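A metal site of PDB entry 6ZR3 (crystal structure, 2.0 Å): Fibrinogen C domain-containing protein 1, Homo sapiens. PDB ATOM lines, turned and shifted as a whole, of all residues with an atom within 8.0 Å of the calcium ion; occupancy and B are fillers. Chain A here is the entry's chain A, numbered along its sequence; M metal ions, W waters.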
ATOM      1  N   THR A 153       2.380   3.309  -5.898  1.00  0.00           N
ATOM      2  CA  THR A 153       1.154   3.524  -5.076  1.00  0.00           C
ATOM      3  C   THR A 153       0.800   5.010  -5.031  1.00  0.00           C
ATOM      4  O   THR A 153       1.696   5.845  -4.817  1.00  0.00           O
ATOM      5  CB  THR A 153       1.365   2.894  -3.695  1.00  0.00           C
ATOM      6  OG1 THR A 153       1.207   1.477  -3.845  1.00  0.00           O
ATOM      7  CG2 THR A 153       0.388   3.392  -2.654  1.00  0.00           C
ATOM      8  N   ARG A 157      -4.919   4.197  -5.149  1.00  0.00           N
ATOM      9  CA  ARG A 157      -4.546   2.857  -5.685  1.00  0.00           C
ATOM     10  C   ARG A 157      -3.378   2.285  -4.889  1.00  0.00           C
ATOM     11  O   ARG A 157      -2.220   2.680  -5.146  1.00  0.00           O
ATOM     12  CB  ARG A 157      -4.226   2.926  -7.179  1.00  0.00           C
ATOM     13  CG  ARG A 157      -4.321   1.576  -7.890  1.00  0.00           C
ATOM     14  CD  ARG A 157      -4.012   1.706  -9.367  1.00  0.00           C
ATOM     15  NE  ARG A 157      -4.255   0.468 -10.113  1.00  0.00           N
ATOM     16  CZ  ARG A 157      -3.412  -0.559 -10.193  1.00  0.00           C
ATOM     17  NH1 ARG A 157      -2.243  -0.542  -9.556  1.00  0.00           N
ATOM     18  NH2 ARG A 157      -3.740  -1.625 -10.899  1.00  0.00           N
ATOM     19  N   ASP A 158      -3.691   1.363  -3.977  1.00  0.00           N
ATOM     20  CA  ASP A 158      -2.770   0.844  -2.933  1.00  0.00           C
ATOM     21  C   ASP A 158      -2.221  -0.519  -3.377  1.00  0.00           C
ATOM     22  O   ASP A 158      -3.014  -1.483  -3.403  1.00  0.00           O
ATOM     23  CB  ASP A 158      -3.521   0.779  -1.603  1.00  0.00           C
ATOM     24  CG  ASP A 158      -2.696   0.239  -0.456  1.00  0.00           C
ATOM     25  OD1 ASP A 158      -1.543  -0.196  -0.712  1.00  0.00           O
ATOM     26  OD2 ASP A 158      -3.207   0.245   0.689  1.00  0.00           O
ATOM     27  N   SER A 159      -0.926  -0.601  -3.677  1.00  0.00           N
ATOM     28  CA  SER A 159      -0.184  -1.846  -4.028  1.00  0.00           C
ATOM     29  C   SER A 159       1.041  -2.022  -3.134  1.00  0.00           C
ATOM     30  O   SER A 159       1.931  -2.792  -3.525  1.00  0.00           O
ATOM     31  CB  SER A 159       0.232  -1.850  -5.482  1.00  0.00           C
ATOM     32  OG  SER A 159      -0.860  -1.558  -6.342  1.00  0.00           O
ATOM     33  N   ASP A 160       1.099  -1.329  -1.989  1.00  0.00           N
ATOM     34  CA  ASP A 160       2.307  -1.263  -1.115  1.00  0.00           C
ATOM     35  C   ASP A 160       2.308  -2.459  -0.154  1.00  0.00           C
ATOM     36  O   ASP A 160       1.427  -3.337  -0.311  1.00  0.00           O
ATOM     37  CB  ASP A 160       2.402   0.085  -0.391  1.00  0.00           C
ATOM     38  CG  ASP A 160       1.261   0.333   0.588  1.00  0.00           C
ATOM     39  OD1 ASP A 160       0.886  -0.611   1.310  1.00  0.00           O
ATOM     40  OD2 ASP A 160       0.743   1.471   0.598  1.00  0.00           O
ATOM     41  N   HIS A 161       3.257  -2.487   0.801  1.00  0.00           N
ATOM     42  CA  HIS A 161       3.430  -3.556   1.820  1.00  0.00           C
ATOM     43  C   HIS A 161       3.164  -3.017   3.237  1.00  0.00           C
ATOM     44  O   HIS A 161       3.668  -3.630   4.202  1.00  0.00           O
ATOM     45  CB  HIS A 161       4.823  -4.196   1.708  1.00  0.00           C
ATOM     46  CG  HIS A 161       4.963  -5.125   0.551  1.00  0.00           C
ATOM     47  ND1 HIS A 161       6.183  -5.670   0.208  1.00  0.00           N
ATOM     48  CD2 HIS A 161       4.069  -5.600  -0.331  1.00  0.00           C
ATOM     49  CE1 HIS A 161       6.026  -6.452  -0.853  1.00  0.00           C
ATOM     50  NE2 HIS A 161       4.738  -6.424  -1.198  1.00  0.00           N
ATOM     51  N   SER A 162       2.417  -1.930   3.356  1.00  0.00           N
ATOM     52  CA  SER A 162       1.759  -1.508   4.620  1.00  0.00           C
ATOM     53  C   SER A 162       0.322  -2.062   4.612  1.00  0.00           C
ATOM     54  O   SER A 162      -0.168  -2.374   3.511  1.00  0.00           O
ATOM     55  CB  SER A 162       1.759  -0.006   4.780  1.00  0.00           C
ATOM     56  OG  SER A 162       0.867   0.399   5.808  1.00  0.00           O
ATOM     57  N   GLU A 163      -0.303  -2.185   5.785  1.00  0.00           N
ATOM     58  CA  GLU A 163      -1.758  -2.460   5.912  1.00  0.00           C
ATOM     59  C   GLU A 163      -2.511  -1.130   5.797  1.00  0.00           C
ATOM     60  O   GLU A 163      -3.744  -1.174   5.663  1.00  0.00           O
ATOM     61  CB  GLU A 163      -2.034  -3.221   7.200  1.00  0.00           C
ATOM     62  CG  GLU A 163      -1.819  -4.721   7.058  1.00  0.00           C
ATOM     63  CD  GLU A 163      -1.170  -5.422   8.242  1.00  0.00           C
ATOM     64  OE1 GLU A 163      -0.896  -4.754   9.251  1.00  0.00           O
ATOM     65  OE2 GLU A 163      -0.947  -6.654   8.149  1.00  0.00           O
ATOM     66  N   ASN A 164      -1.796   0.008   5.841  1.00  0.00           N
ATOM     67  CA  ASN A 164      -2.298   1.360   5.454  1.00  0.00           C
ATOM     68  C   ASN A 164      -1.951   1.636   3.986  1.00  0.00           C
ATOM     69  O   ASN A 164      -1.278   0.783   3.364  1.00  0.00           O
ATOM     70  CB  ASN A 164      -1.681   2.469   6.308  1.00  0.00           C
ATOM     71  CG  ASN A 164      -1.943   2.320   7.790  1.00  0.00           C
ATOM     72  OD1 ASN A 164      -3.008   1.866   8.197  1.00  0.00           O
ATOM     73  ND2 ASN A 164      -0.977   2.712   8.603  1.00  0.00           N
ATOM     74  N   ASN A 165      -2.401   2.777   3.453  1.00  0.00           N
ATOM     75  CA  ASN A 165      -1.982   3.317   2.126  1.00  0.00           C
ATOM     76  C   ASN A 165      -0.806   4.285   2.380  1.00  0.00           C
ATOM     77  O   ASN A 165      -1.057   5.409   2.857  1.00  0.00           O
ATOM     78  CB  ASN A 165      -3.152   3.962   1.384  1.00  0.00           C
ATOM     79  CG  ASN A 165      -2.800   4.441  -0.011  1.00  0.00           C
ATOM     80  OD1 ASN A 165      -1.758   5.054  -0.229  1.00  0.00           O
ATOM     81  ND2 ASN A 165      -3.675   4.181  -0.974  1.00  0.00           N
ATOM     82  N   CYS A 166       0.424   3.847   2.060  1.00  0.00           N
ATOM     83  CA  CYS A 166       1.694   4.604   2.255  1.00  0.00           C
ATOM     84  C   CYS A 166       1.631   5.980   1.586  1.00  0.00           C
ATOM     85  O   CYS A 166       2.197   6.925   2.162  1.00  0.00           O
ATOM     86  CB  CYS A 166       2.899   3.849   1.700  1.00  0.00           C
ATOM     87  SG  CYS A 166       3.344   2.341   2.613  1.00  0.00           S
ATOM     88  N   ALA A 167       0.986   6.085   0.411  1.00  0.00           N
ATOM     89  CA  ALA A 167       0.852   7.339  -0.386  1.00  0.00           C
ATOM     90  C   ALA A 167      -0.046   8.346   0.335  1.00  0.00           C
ATOM     91  O   ALA A 167       0.323   9.519   0.385  1.00  0.00           O
ATOM     92  CB  ALA A 167       0.324   7.026  -1.766  1.00  0.00           C
ATOM     93  N   TYR A 176       6.266   2.421  -3.031  1.00  0.00           N
ATOM     94  CA  TYR A 176       6.250   2.244  -1.556  1.00  0.00           C
ATOM     95  C   TYR A 176       6.353   0.773  -1.173  1.00  0.00           C
ATOM     96  O   TYR A 176       5.664  -0.085  -1.788  1.00  0.00           O
ATOM     97  CB  TYR A 176       4.956   2.800  -0.947  1.00  0.00           C
ATOM     98  CG  TYR A 176       4.876   4.299  -0.939  1.00  0.00           C
ATOM     99  CD1 TYR A 176       5.822   5.064  -0.263  1.00  0.00           C
ATOM    100  CD2 TYR A 176       3.868   4.969  -1.618  1.00  0.00           C
ATOM    101  CE1 TYR A 176       5.759   6.448  -0.265  1.00  0.00           C
ATOM    102  CE2 TYR A 176       3.783   6.346  -1.615  1.00  0.00           C
ATOM    103  CZ  TYR A 176       4.732   7.090  -0.934  1.00  0.00           C
ATOM    104  OH  TYR A 176       4.637   8.451  -0.955  1.00  0.00           O
ATOM    105  N   ARG A 177       7.166   0.522  -0.154  1.00  0.00           N
ATOM    106  CA  ARG A 177       7.324  -0.797   0.512  1.00  0.00           C
ATOM    107  C   ARG A 177       6.556  -0.747   1.838  1.00  0.00           C
ATOM    108  O   ARG A 177       5.340  -1.046   1.808  1.00  0.00           O
ATOM    109  CB  ARG A 177       8.819  -1.131   0.627  1.00  0.00           C
ATOM    110  CG  ARG A 177       9.093  -2.522   1.169  1.00  0.00           C
ATOM    111  CD  ARG A 177      10.549  -2.907   1.133  1.00  0.00           C
ATOM    112  NE  ARG A 177      10.672  -4.295   1.551  1.00  0.00           N
ATOM    113  CZ  ARG A 177      10.437  -5.354   0.769  1.00  0.00           C
ATOM    114  NH1 ARG A 177      10.073  -5.189  -0.493  1.00  0.00           N
ATOM    115  NH2 ARG A 177      10.558  -6.577   1.255  1.00  0.00           N
ATOM    116  N   ASN A 178       7.198  -0.336   2.935  1.00  0.00           N
ATOM    117  CA  ASN A 178       6.563  -0.259   4.282  1.00  0.00           C
ATOM    118  C   ASN A 178       7.334   0.692   5.192  1.00  0.00           C
ATOM    119  O   ASN A 178       7.772   0.290   6.260  1.00  0.00           O
ATOM    120  CB  ASN A 178       6.471  -1.663   4.894  1.00  0.00           C
ATOM    121  CG  ASN A 178       5.545  -1.738   6.077  1.00  0.00           C
ATOM    122  OD1 ASN A 178       4.580  -0.979   6.164  1.00  0.00           O
ATOM    123  ND2 ASN A 178       5.812  -2.663   6.990  1.00  0.00           N
ATOM    124  N   CYS A 179       7.492   1.960   4.789  1.00  0.00           N
ATOM    125  CA  CYS A 179       6.905   2.511   3.583  1.00  0.00           C
ATOM    126  C   CYS A 179       7.979   3.049   2.632  1.00  0.00           C
ATOM    127  O   CYS A 179       7.840   2.788   1.430  1.00  0.00           O
ATOM    128  CB  CYS A 179       5.872   3.592   3.912  1.00  0.00           C
ATOM    129  SG  CYS A 179       4.256   2.921   4.377  1.00  0.00           S
HETATM  130 CA    CA M   1      -1.386  -0.993   1.722  1.00  0.00          CA
HETATM  131  O   HOH W   1      -3.675  -1.932   2.249  1.00  0.00           O
HETATM  132  O   HOH W   2      -1.143  -3.232   0.451  1.00  0.00           O
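O of Arg 177 is in hydrogen-bond range of N of Ser 162 (3.4 Å). SG of Cys 166 is disulfide-bonded to SG of Cys 179, at 2.1 Å. The side-chain hydroxyl of Ser 162 sits at hydrogen-bond distance from the backbone NH of Asn 164, 2.7 Å away. The backbone NH (N) of Asp 160 sits at hydrogen-bond distance from the side-chain hydroxyl (OG1) of Thr 153, at 3.4 Å. N of Cys 166 lies within hydrogen-bond range of OD2 of Asp 160 (2.8 Å).
Of the 16 residues printed, 4 come within 4 Å of the calcium ion. The nearest printed residue that does not touch the calcium ion is Glu 163 (4.2 Å).
The calcium ion is bound by OD1 of Asp 160 (2.3 Å), O of Asn 164 (2.4 Å), OD2 of Asp 158 (2.4 Å), water W1 (2.5 Å), OD1 of Asp 158 (2.6 Å), O of Ser 162 (2.6 Å) and water W2 (2.6 Å). The calcium ion has seven donor atoms within binding distance.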
